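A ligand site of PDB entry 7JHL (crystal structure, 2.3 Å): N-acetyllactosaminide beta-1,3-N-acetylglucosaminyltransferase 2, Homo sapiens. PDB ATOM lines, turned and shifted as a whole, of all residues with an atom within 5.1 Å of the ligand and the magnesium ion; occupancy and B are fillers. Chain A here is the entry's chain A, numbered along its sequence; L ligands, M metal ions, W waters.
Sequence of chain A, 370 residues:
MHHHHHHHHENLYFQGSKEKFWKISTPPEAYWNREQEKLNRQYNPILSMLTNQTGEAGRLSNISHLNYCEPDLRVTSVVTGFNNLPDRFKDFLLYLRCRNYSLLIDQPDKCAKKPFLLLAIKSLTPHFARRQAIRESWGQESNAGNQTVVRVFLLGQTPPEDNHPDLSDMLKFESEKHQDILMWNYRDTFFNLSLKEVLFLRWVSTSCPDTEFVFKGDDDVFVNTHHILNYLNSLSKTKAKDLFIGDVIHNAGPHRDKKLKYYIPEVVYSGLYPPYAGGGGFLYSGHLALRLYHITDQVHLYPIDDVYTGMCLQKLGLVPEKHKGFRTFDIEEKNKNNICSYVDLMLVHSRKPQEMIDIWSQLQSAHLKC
NZ of Lys 196 lies within hydrogen-bond range of O7 of the ligand (2.6 Å). OD1 of Asp 305 sits at hydrogen-bond distance from O3 of the ligand. The side-chain carboxylate of Asp 188 sits at hydrogen-bond distance from a nitrogen (N3) of the ligand, 2.7 Å away. The side-chain hydroxyl of Tyr 262 sits at hydrogen-bond distance from an oxygen (O17) of the ligand (2.8 Å). An oxygen (O2) of the ligand lies close to the backbone carbonyl oxygen of Gly 279 (3.1 Å). O11 of the ligand sits at hydrogen-bond distance from O of Lys 122 (3.0 Å). The side-chain amino group (NZ) of Lys 122 is in hydrogen-bond range of an oxygen (O3) of the ligand, 2.9 Å away. N of Asp 219 lies within hydrogen-bond range of O11 of the ligand (2.9 Å). An oxygen (O9) of the ligand lies within hydrogen-bond range of the side-chain carboxylate of Asp 219 (2.9 Å). OD2 of Asp 218 sits at hydrogen-bond distance from O2 of the ligand (3.0 Å). The backbone NH of Thr 189 sits close to an oxygen (O8) of the ligand (3.5 Å). N of Phe 190 is in hydrogen-bond range of O8 of the ligand (3.3 Å). The backbone NH (N) of Gly 280 lies within hydrogen-bond range of an oxygen (O2) of the ligand (3.3 Å). The side-chain amino group (NZ) of Lys 261 lies within salt-bridge range of an oxygen (O17) of the ligand (3.4 Å).
NZ of Lys 196 lies within hydrogen-bond range of O of Ser 123, at 3.0 Å. The side-chain amino group of Lys 196 sits at hydrogen-bond distance from the backbone carbonyl oxygen of Leu 154 (3.0 Å). The side-chain carboxylate (OD2) of Asp 305 is in salt-bridge range of the side-chain amino group (NZ) of Lys 122, 2.9 Å away. The backbone NH (N) of Gly 279 lies within hydrogen-bond range of the side-chain carboxylate (OD2) of Asp 306 (2.8 Å). OD1 of Asp 218 is in salt-bridge range of NZ of Lys 122. N of Lys 122 lies within hydrogen-bond range of O of Gly 217 (3.0 Å). NH1 of Arg 130 lies within salt-bridge range of OD1 of Asp 219, at 2.9 Å. The backbone carbonyl oxygen (O) of Gly 280 is in hydrogen-bond range of the backbone NH (N) of Asp 218.
An oxygen (O7) of the ligand sits close to the backbone carbonyl oxygen of Ser 123 (3.4 Å). Leu 124 touches the ligand (CG to N3, 3.5 Å). ND1 of His 127 touches O9 of the ligand, 3.6 Å away. Leu 193 touches the ligand. Hydrophobic or aromatic side chains that line the ligand: Leu 124, His 127, Phe 190, Leu 193, Tyr 262 and His 349. Of the 27 residues printed, 18 come within 4 Å of the ligand. The nearest printed residue that does not touch the ligand is Asp 306 (4.04 Å).
Of the 27 residues printed, 2 come within 4 Å of the magnesium ion. The nearest printed residue that does not touch the magnesium ion is Asp 218 (4.4 Å).
The magnesium ion is bound by O16 of the ligand, 2.1 Å away. Water W3 binds the magnesium ion (2.2 Å). The magnesium ion is bound by OD2 of Asp 220. The magnesium ion is bound by water W4, 2.2 Å away. NE2 of His 349 binds the magnesium ion. O14 of the ligand is bound to the magnesium ion (2.2 Å).
Water W4 bridges OD1 of Asp 220 (2.6 Å) and N1 of the ligand (3.4 Å). Water W2 lies within hydrogen-bond range of an oxygen (O13) of the ligand and the guanidinium group of Arg 130. Water W5 lies within hydrogen-bond range of O of Pro 303 (2.7 Å), O of Phe 190 (2.7 Å), N of Asp 305 (3.1 Å) and O5 of the ligand (3.2 Å).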
ATOM      1  N   LYS A 122       1.587 -28.744   0.262  1.00  0.00           N
ATOM      2  CA  LYS A 122       0.544 -28.516   1.258  1.00  0.00           C
ATOM      3  C   LYS A 122      -0.823 -28.506   0.599  1.00  0.00           C
ATOM      4  O   LYS A 122      -1.037 -27.807  -0.398  1.00  0.00           O
ATOM      5  CB  LYS A 122       0.790 -27.197   1.984  1.00  0.00           C
ATOM      6  CG  LYS A 122       2.109 -27.130   2.695  1.00  0.00           C
ATOM      7  CD  LYS A 122       2.302 -25.769   3.324  1.00  0.00           C
ATOM      8  CE  LYS A 122       2.532 -24.723   2.274  1.00  0.00           C
ATOM      9  NZ  LYS A 122       2.460 -23.329   2.821  1.00  0.00           N
ATOM     10  N   SER A 123      -1.757 -29.269   1.153  1.00  0.00           N
ATOM     11  CA  SER A 123      -3.079 -29.362   0.554  1.00  0.00           C
ATOM     12  C   SER A 123      -4.124 -29.522   1.651  1.00  0.00           C
ATOM     13  O   SER A 123      -3.822 -29.853   2.791  1.00  0.00           O
ATOM     14  CB  SER A 123      -3.148 -30.518  -0.452  1.00  0.00           C
ATOM     15  OG  SER A 123      -4.215 -30.335  -1.369  1.00  0.00           O
ATOM     16  N   LEU A 124      -5.363 -29.244   1.266  1.00  0.00           N
ATOM     17  CA  LEU A 124      -6.534 -29.471   2.104  1.00  0.00           C
ATOM     18  C   LEU A 124      -7.377 -30.587   1.487  1.00  0.00           C
ATOM     19  O   LEU A 124      -7.469 -30.712   0.263  1.00  0.00           O
ATOM     20  CB  LEU A 124      -7.385 -28.197   2.222  1.00  0.00           C
ATOM     21  CG  LEU A 124      -7.085 -27.240   3.356  1.00  0.00           C
ATOM     22  CD1 LEU A 124      -7.746 -25.899   3.078  1.00  0.00           C
ATOM     23  CD2 LEU A 124      -7.602 -27.817   4.656  1.00  0.00           C
ATOM     24  N   HIS A 127      -9.350 -30.514  -1.887  1.00  0.00           N
ATOM     25  CA  HIS A 127      -8.667 -30.061  -3.095  1.00  0.00           C
ATOM     26  C   HIS A 127      -8.285 -31.207  -4.015  1.00  0.00           C
ATOM     27  O   HIS A 127      -7.117 -31.326  -4.421  1.00  0.00           O
ATOM     28  CB  HIS A 127      -7.410 -29.256  -2.722  1.00  0.00           C
ATOM     29  CG  HIS A 127      -7.702 -27.966  -2.024  1.00  0.00           C
ATOM     30  ND1 HIS A 127      -6.708 -27.122  -1.572  1.00  0.00           N
ATOM     31  CD2 HIS A 127      -8.878 -27.366  -1.701  1.00  0.00           C
ATOM     32  CE1 HIS A 127      -7.254 -26.062  -0.988  1.00  0.00           C
ATOM     33  NE2 HIS A 127      -8.572 -26.187  -1.065  1.00  0.00           N
ATOM     34  N   ARG A 130      -6.936 -30.087  -7.510  1.00  0.00           N
ATOM     35  CA  ARG A 130      -5.596 -29.513  -7.468  1.00  0.00           C
ATOM     36  C   ARG A 130      -4.541 -30.600  -7.396  1.00  0.00           C
ATOM     37  O   ARG A 130      -3.530 -30.553  -8.107  1.00  0.00           O
ATOM     38  CB  ARG A 130      -5.453 -28.560  -6.281  1.00  0.00           C
ATOM     39  CG  ARG A 130      -6.308 -27.302  -6.332  1.00  0.00           C
ATOM     40  CD  ARG A 130      -5.919 -26.335  -5.236  1.00  0.00           C
ATOM     41  NE  ARG A 130      -6.939 -25.312  -5.017  1.00  0.00           N
ATOM     42  CZ  ARG A 130      -6.823 -24.288  -4.162  1.00  0.00           C
ATOM     43  NH1 ARG A 130      -5.716 -24.129  -3.437  1.00  0.00           N
ATOM     44  NH2 ARG A 130      -7.816 -23.422  -4.040  1.00  0.00           N
ATOM     45  N   LEU A 154       0.586 -32.995   1.803  1.00  0.00           N
ATOM     46  CA  LEU A 154       0.587 -32.842   3.254  1.00  0.00           C
ATOM     47  C   LEU A 154      -0.782 -32.341   3.694  1.00  0.00           C
ATOM     48  O   LEU A 154      -1.162 -31.198   3.400  1.00  0.00           O
ATOM     49  CB  LEU A 154       1.684 -31.869   3.684  1.00  0.00           C
ATOM     50  CG  LEU A 154       3.081 -32.077   3.103  1.00  0.00           C
ATOM     51  CD1 LEU A 154       3.983 -30.914   3.503  1.00  0.00           C
ATOM     52  CD2 LEU A 154       3.664 -33.415   3.548  1.00  0.00           C
ATOM     53  N   ASP A 188      -6.590 -29.052  10.273  1.00  0.00           N
ATOM     54  CA  ASP A 188      -5.913 -28.343   9.188  1.00  0.00           C
ATOM     55  C   ASP A 188      -6.520 -26.952   9.034  1.00  0.00           C
ATOM     56  O   ASP A 188      -7.640 -26.810   8.533  1.00  0.00           O
ATOM     57  CB  ASP A 188      -6.047 -29.130   7.886  1.00  0.00           C
ATOM     58  CG  ASP A 188      -4.920 -28.834   6.899  1.00  0.00           C
ATOM     59  OD1 ASP A 188      -4.291 -27.756   7.001  1.00  0.00           O
ATOM     60  OD2 ASP A 188      -4.697 -29.672   6.003  1.00  0.00           O
ATOM     61  N   THR A 189      -5.799 -25.921   9.482  1.00  0.00           N
ATOM     62  CA  THR A 189      -6.231 -24.535   9.375  1.00  0.00           C
ATOM     63  C   THR A 189      -5.034 -23.680   8.999  1.00  0.00           C
ATOM     64  O   THR A 189      -3.883 -24.122   9.085  1.00  0.00           O
ATOM     65  CB  THR A 189      -6.839 -24.006  10.680  1.00  0.00           C
ATOM     66  OG1 THR A 189      -5.850 -24.046  11.720  1.00  0.00           O
ATOM     67  CG2 THR A 189      -8.080 -24.834  11.109  1.00  0.00           C
ATOM     68  N   PHE A 190      -5.299 -22.431   8.612  1.00  0.00           N
ATOM     69  CA  PHE A 190      -4.207 -21.526   8.253  1.00  0.00           C
ATOM     70  C   PHE A 190      -3.245 -21.327   9.418  1.00  0.00           C
ATOM     71  O   PHE A 190      -2.021 -21.353   9.236  1.00  0.00           O
ATOM     72  CB  PHE A 190      -4.750 -20.173   7.774  1.00  0.00           C
ATOM     73  CG  PHE A 190      -4.994 -20.111   6.286  1.00  0.00           C
ATOM     74  CD1 PHE A 190      -3.927 -20.077   5.401  1.00  0.00           C
ATOM     75  CD2 PHE A 190      -6.289 -20.093   5.782  1.00  0.00           C
ATOM     76  CE1 PHE A 190      -4.133 -20.025   4.031  1.00  0.00           C
ATOM     77  CE2 PHE A 190      -6.515 -20.040   4.403  1.00  0.00           C
ATOM     78  CZ  PHE A 190      -5.438 -20.016   3.528  1.00  0.00           C
ATOM     79  N   LEU A 193      -0.554 -24.091  10.065  1.00  0.00           N
ATOM     80  CA  LEU A 193       0.345 -24.480   8.974  1.00  0.00           C
ATOM     81  C   LEU A 193       1.797 -24.616   9.440  1.00  0.00           C
ATOM     82  O   LEU A 193       2.552 -25.394   8.853  1.00  0.00           O
ATOM     83  CB  LEU A 193       0.230 -23.484   7.821  1.00  0.00           C
ATOM     84  CG  LEU A 193      -1.000 -23.647   6.926  1.00  0.00           C
ATOM     85  CD1 LEU A 193      -1.020 -22.568   5.853  1.00  0.00           C
ATOM     86  CD2 LEU A 193      -1.025 -25.035   6.295  1.00  0.00           C
ATOM     87  N   LYS A 196       1.963 -27.975  10.415  1.00  0.00           N
ATOM     88  CA  LYS A 196       2.145 -28.829   9.252  1.00  0.00           C
ATOM     89  C   LYS A 196       3.611 -28.877   8.831  1.00  0.00           C
ATOM     90  O   LYS A 196       4.108 -29.927   8.391  1.00  0.00           O
ATOM     91  CB  LYS A 196       1.263 -28.341   8.101  1.00  0.00           C
ATOM     92  CG  LYS A 196       1.294 -29.243   6.870  1.00  0.00           C
ATOM     93  CD  LYS A 196       0.315 -28.774   5.787  1.00  0.00           C
ATOM     94  CE  LYS A 196      -1.136 -28.988   6.225  1.00  0.00           C
ATOM     95  NZ  LYS A 196      -2.088 -28.915   5.091  1.00  0.00           N
ATOM     96  N   GLY A 217       5.921 -26.472  -1.335  1.00  0.00           N
ATOM     97  CA  GLY A 217       5.117 -25.419  -1.926  1.00  0.00           C
ATOM     98  C   GLY A 217       3.636 -25.658  -1.727  1.00  0.00           C
ATOM     99  O   GLY A 217       3.226 -26.610  -1.067  1.00  0.00           O
ATOM    100  N   ASP A 218       2.847 -24.767  -2.314  1.00  0.00           N
ATOM    101  CA  ASP A 218       1.400 -24.784  -2.234  1.00  0.00           C
ATOM    102  C   ASP A 218       0.801 -25.600  -3.379  1.00  0.00           C
ATOM    103  O   ASP A 218       1.480 -25.963  -4.343  1.00  0.00           O
ATOM    104  CB  ASP A 218       0.847 -23.353  -2.262  1.00  0.00           C
ATOM    105  CG  ASP A 218       1.329 -22.504  -1.109  1.00  0.00           C
ATOM    106  OD1 ASP A 218       1.820 -23.059  -0.097  1.00  0.00           O
ATOM    107  OD2 ASP A 218       1.216 -21.260  -1.196  1.00  0.00           O
ATOM    108  N   ASP A 219      -0.499 -25.872  -3.283  1.00  0.00           N
ATOM    109  CA  ASP A 219      -1.177 -26.647  -4.323  1.00  0.00           C
ATOM    110  C   ASP A 219      -1.850 -25.764  -5.370  1.00  0.00           C
ATOM    111  O   ASP A 219      -2.597 -26.273  -6.202  1.00  0.00           O
ATOM    112  CB  ASP A 219      -2.168 -27.633  -3.698  1.00  0.00           C
ATOM    113  CG  ASP A 219      -3.314 -26.951  -2.938  1.00  0.00           C
ATOM    114  OD1 ASP A 219      -3.352 -25.706  -2.830  1.00  0.00           O
ATOM    115  OD2 ASP A 219      -4.177 -27.692  -2.420  1.00  0.00           O
ATOM    116  N   ASP A 220      -1.577 -24.463  -5.358  1.00  0.00           N
ATOM    117  CA  ASP A 220      -2.096 -23.564  -6.387  1.00  0.00           C
ATOM    118  C   ASP A 220      -0.974 -22.867  -7.164  1.00  0.00           C
ATOM    119  O   ASP A 220      -1.187 -21.780  -7.711  1.00  0.00           O
ATOM    120  CB  ASP A 220      -3.024 -22.525  -5.754  1.00  0.00           C
ATOM    121  CG  ASP A 220      -2.315 -21.624  -4.750  1.00  0.00           C
ATOM    122  OD1 ASP A 220      -1.190 -21.970  -4.324  1.00  0.00           O
ATOM    123  OD2 ASP A 220      -2.888 -20.569  -4.385  1.00  0.00           O
ATOM    124  N   LYS A 261      -5.719 -10.503   6.159  1.00  0.00           N
ATOM    125  CA  LYS A 261      -5.586 -11.937   6.370  1.00  0.00           C
ATOM    126  C   LYS A 261      -4.440 -12.256   7.326  1.00  0.00           C
ATOM    127  O   LYS A 261      -4.544 -13.182   8.142  1.00  0.00           O
ATOM    128  CB  LYS A 261      -5.383 -12.648   5.030  1.00  0.00           C
ATOM    129  CG  LYS A 261      -5.602 -14.153   5.070  1.00  0.00           C
ATOM    130  CD  LYS A 261      -4.581 -14.888   4.190  1.00  0.00           C
ATOM    131  CE  LYS A 261      -4.890 -16.370   4.075  1.00  0.00           C
ATOM    132  NZ  LYS A 261      -5.243 -16.758   2.678  1.00  0.00           N
ATOM    133  N   TYR A 262      -3.341 -11.502   7.251  1.00  0.00           N
ATOM    134  CA  TYR A 262      -2.157 -11.739   8.070  1.00  0.00           C
ATOM    135  C   TYR A 262      -2.075 -10.780   9.251  1.00  0.00           C
ATOM    136  O   TYR A 262      -0.979 -10.429   9.690  1.00  0.00           O
ATOM    137  CB  TYR A 262      -0.901 -11.652   7.210  1.00  0.00           C
ATOM    138  CG  TYR A 262      -0.987 -12.512   5.977  1.00  0.00           C
ATOM    139  CD1 TYR A 262      -1.078 -13.887   6.073  1.00  0.00           C
ATOM    140  CD2 TYR A 262      -1.001 -11.933   4.707  1.00  0.00           C
ATOM    141  CE1 TYR A 262      -1.170 -14.683   4.949  1.00  0.00           C
ATOM    142  CE2 TYR A 262      -1.102 -12.717   3.584  1.00  0.00           C
ATOM    143  CZ  TYR A 262      -1.181 -14.093   3.709  1.00  0.00           C
ATOM    144  OH  TYR A 262      -1.281 -14.867   2.575  1.00  0.00           O
ATOM    145  N   GLY A 278       8.744 -16.540   0.717  1.00  0.00           N
ATOM    146  CA  GLY A 278       7.314 -16.689   0.519  1.00  0.00           C
ATOM    147  C   GLY A 278       6.931 -18.151   0.469  1.00  0.00           C
ATOM    148  O   GLY A 278       7.599 -18.944  -0.191  1.00  0.00           O
ATOM    149  N   GLY A 279       5.868 -18.514   1.172  1.00  0.00           N
ATOM    150  CA  GLY A 279       5.536 -19.914   1.317  1.00  0.00           C
ATOM    151  C   GLY A 279       5.024 -20.583   0.061  1.00  0.00           C
ATOM    152  O   GLY A 279       4.899 -21.817   0.055  1.00  0.00           O
ATOM    153  N   GLY A 280       4.723 -19.807  -0.992  1.00  0.00           N
ATOM    154  CA  GLY A 280       4.260 -20.399  -2.234  1.00  0.00           C
ATOM    155  C   GLY A 280       5.139 -21.537  -2.700  1.00  0.00           C
ATOM    156  O   GLY A 280       4.655 -22.497  -3.318  1.00  0.00           O
ATOM    157  N   PRO A 303       1.737 -18.227  13.888  1.00  0.00           N
ATOM    158  CA  PRO A 303       0.539 -18.401  13.041  1.00  0.00           C
ATOM    159  C   PRO A 303       0.811 -18.320  11.553  1.00  0.00           C
ATOM    160  O   PRO A 303      -0.046 -18.757  10.768  1.00  0.00           O
ATOM    161  CB  PRO A 303      -0.381 -17.259  13.490  1.00  0.00           C
ATOM    162  CG  PRO A 303       0.053 -16.951  14.873  1.00  0.00           C
ATOM    163  CD  PRO A 303       1.545 -17.147  14.875  1.00  0.00           C
ATOM    164  N   ILE A 304       1.943 -17.773  11.121  1.00  0.00           N
ATOM    165  CA  ILE A 304       2.274 -17.665   9.708  1.00  0.00           C
ATOM    166  C   ILE A 304       3.428 -18.622   9.437  1.00  0.00           C
ATOM    167  O   ILE A 304       4.542 -18.432   9.939  1.00  0.00           O
ATOM    168  CB  ILE A 304       2.632 -16.226   9.319  1.00  0.00           C
ATOM    169  CG1 ILE A 304       1.571 -15.267   9.884  1.00  0.00           C
ATOM    170  CG2 ILE A 304       2.688 -16.094   7.826  1.00  0.00           C
ATOM    171  CD1 ILE A 304       1.788 -13.825   9.485  1.00  0.00           C
ATOM    172  N   ASP A 305       3.164 -19.661   8.633  1.00  0.00           N
ATOM    173  CA  ASP A 305       4.072 -20.798   8.567  1.00  0.00           C
ATOM    174  C   ASP A 305       5.401 -20.429   7.903  1.00  0.00           C
ATOM    175  O   ASP A 305       6.450 -20.919   8.319  1.00  0.00           O
ATOM    176  CB  ASP A 305       3.408 -21.965   7.847  1.00  0.00           C
ATOM    177  CG  ASP A 305       3.081 -21.654   6.389  1.00  0.00           C
ATOM    178  OD1 ASP A 305       2.781 -20.490   6.057  1.00  0.00           O
ATOM    179  OD2 ASP A 305       3.127 -22.593   5.559  1.00  0.00           O
ATOM    180  N   ASP A 306       5.371 -19.578   6.878  1.00  0.00           N
ATOM    181  CA  ASP A 306       6.639 -19.233   6.230  1.00  0.00           C
ATOM    182  C   ASP A 306       7.463 -18.258   7.063  1.00  0.00           C
ATOM    183  O   ASP A 306       8.693 -18.253   6.929  1.00  0.00           O
ATOM    184  CB  ASP A 306       6.408 -18.688   4.808  1.00  0.00           C
ATOM    185  CG  ASP A 306       5.238 -17.732   4.719  1.00  0.00           C
ATOM    186  OD1 ASP A 306       4.770 -17.246   5.774  1.00  0.00           O
ATOM    187  OD2 ASP A 306       4.780 -17.456   3.582  1.00  0.00           O
ATOM    188  N   THR A 328       6.014 -15.308  -6.615  1.00  0.00           N
ATOM    189  CA  THR A 328       4.869 -15.406  -5.733  1.00  0.00           C
ATOM    190  C   THR A 328       3.776 -14.406  -6.080  1.00  0.00           C
ATOM    191  O   THR A 328       2.661 -14.540  -5.570  1.00  0.00           O
ATOM    192  CB  THR A 328       5.328 -15.198  -4.289  1.00  0.00           C
ATOM    193  OG1 THR A 328       6.137 -14.028  -4.213  1.00  0.00           O
ATOM    194  CG2 THR A 328       6.138 -16.397  -3.835  1.00  0.00           C
ATOM    195  N   HIS A 349       2.775 -18.132  -8.988  1.00  0.00           N
ATOM    196  CA  HIS A 349       1.570 -18.186  -8.173  1.00  0.00           C
ATOM    197  C   HIS A 349       0.633 -17.098  -8.704  1.00  0.00           C
ATOM    198  O   HIS A 349       1.089 -15.985  -8.961  1.00  0.00           O
ATOM    199  CB  HIS A 349       1.930 -17.978  -6.701  1.00  0.00           C
ATOM    200  CG  HIS A 349       0.753 -17.810  -5.804  1.00  0.00           C
ATOM    201  ND1 HIS A 349       0.191 -16.579  -5.535  1.00  0.00           N
ATOM    202  CD2 HIS A 349       0.040 -18.710  -5.082  1.00  0.00           C
ATOM    203  CE1 HIS A 349      -0.822 -16.731  -4.701  1.00  0.00           C
ATOM    204  NE2 HIS A 349      -0.929 -18.017  -4.406  1.00  0.00           N
ATOM    205  N   SER A 350      -0.644 -17.412  -8.909  1.00  0.00           N
ATOM    206  CA  SER A 350      -1.235 -18.734  -8.706  1.00  0.00           C
ATOM    207  C   SER A 350      -1.830 -19.286 -10.010  1.00  0.00           C
ATOM    208  O   SER A 350      -2.056 -18.544 -10.957  1.00  0.00           O
ATOM    209  CB  SER A 350      -2.330 -18.669  -7.642  1.00  0.00           C
ATOM    210  OG  SER A 350      -3.334 -17.750  -8.023  1.00  0.00           O
HETATM  211  C1  LIG L   1      -0.062 -17.632   1.698  1.00  0.00           C
HETATM  212  C2  LIG L   1       1.239 -18.280   1.226  1.00  0.00           C
HETATM  213  C3  LIG L   1       1.318 -19.643   1.830  1.00  0.00           C
HETATM  214  C4  LIG L   1       1.354 -19.573   3.331  1.00  0.00           C
HETATM  215  C5  LIG L   1       0.129 -18.820   3.874  1.00  0.00           C
HETATM  216  C6  LIG L   1       0.272 -18.560   5.340  1.00  0.00           C
HETATM  217  C7  LIG L   1       2.113 -17.543  -1.079  1.00  0.00           C
HETATM  218  C8  LIG L   1       2.053 -17.632  -2.597  1.00  0.00           C
HETATM  219  N1  LIG L   1       1.183 -18.367  -0.252  1.00  0.00           N
HETATM  220  O1  LIG L   1      -1.080 -18.471   1.327  1.00  0.00           O
HETATM  221  O2  LIG L   1       2.471 -20.327   1.321  1.00  0.00           O
HETATM  222  O3  LIG L   1       1.391 -20.885   3.857  1.00  0.00           O
HETATM  223  O4  LIG L   1      -0.071 -17.508   3.190  1.00  0.00           O
HETATM  224  O5  LIG L   1      -0.954 -18.100   5.852  1.00  0.00           O
HETATM  225  O6  LIG L   1       2.909 -16.828  -0.547  1.00  0.00           O
HETATM  226  N2  LIG L   1      -3.460 -24.703   2.999  1.00  0.00           N
HETATM  227  C9  LIG L   1      -3.504 -25.841   3.958  1.00  0.00           C
HETATM  228  N3  LIG L   1      -4.420 -25.799   5.150  1.00  0.00           N
HETATM  229  C10 LIG L   1      -5.255 -24.624   5.350  1.00  0.00           C
HETATM  230  C11 LIG L   1      -5.200 -23.487   4.391  1.00  0.00           C
HETATM  231  C12 LIG L   1      -4.293 -23.537   3.220  1.00  0.00           C
HETATM  232  O7  LIG L   1      -2.817 -26.799   3.782  1.00  0.00           O
HETATM  233  O8  LIG L   1      -5.980 -24.590   6.277  1.00  0.00           O
HETATM  234  C13 LIG L   1      -2.633 -24.760   1.975  1.00  0.00           C
HETATM  235  C14 LIG L   1      -3.337 -24.468   0.635  1.00  0.00           C
HETATM  236  O9  LIG L   1      -3.859 -25.725   0.048  1.00  0.00           O
HETATM  237  C15 LIG L   1      -2.368 -23.906  -0.116  1.00  0.00           C
HETATM  238  C16 LIG L   1      -1.440 -23.055   0.923  1.00  0.00           C
HETATM  239  O10 LIG L   1      -1.597 -23.580   2.113  1.00  0.00           O
HETATM  240  O11 LIG L   1      -1.501 -24.887  -0.696  1.00  0.00           O
HETATM  241  C17 LIG L   1      -1.795 -21.582   0.938  1.00  0.00           C
HETATM  242  O12 LIG L   1      -3.200 -21.434   0.950  1.00  0.00           O
HETATM  243  P1  LIG L   1      -3.871 -20.330  -0.104  1.00  0.00           P
HETATM  244  O13 LIG L   1      -5.357 -20.600  -0.214  1.00  0.00           O
HETATM  245  O14 LIG L   1      -3.249 -20.460  -1.482  1.00  0.00           O
HETATM  246  O15 LIG L   1      -3.625 -18.805   0.476  1.00  0.00           O
HETATM  247  P2  LIG L   1      -2.239 -17.912   0.276  1.00  0.00           P
HETATM  248  O16 LIG L   1      -1.740 -18.022  -1.144  1.00  0.00           O
HETATM  249  O17 LIG L   1      -2.553 -16.462   0.610  1.00  0.00           O
HETATM  250 MG    MG M   1      -2.235 -19.052  -2.913  1.00  0.00          MG
HETATM  251  O   HOH W   1      -6.590 -22.541   0.627  1.00  0.00           O
HETATM  252  O   HOH W   2      -5.558 -20.708  -3.506  1.00  0.00           O
HETATM  253  O   HOH W   3      -3.944 -17.775  -3.381  1.00  0.00           O
HETATM  254  O   HOH W   4      -0.569 -20.413  -2.379  1.00  0.00           O
HETATM  255  O   HOH W   5       0.075 -19.873   8.302  1.00  0.00           O
HETATM  256  O   HOH W   6      -8.469 -23.630   6.048  1.00  0.00           O
HETATM  257  O   HOH W   7      -5.345 -17.019  -1.259  1.00  0.00           O
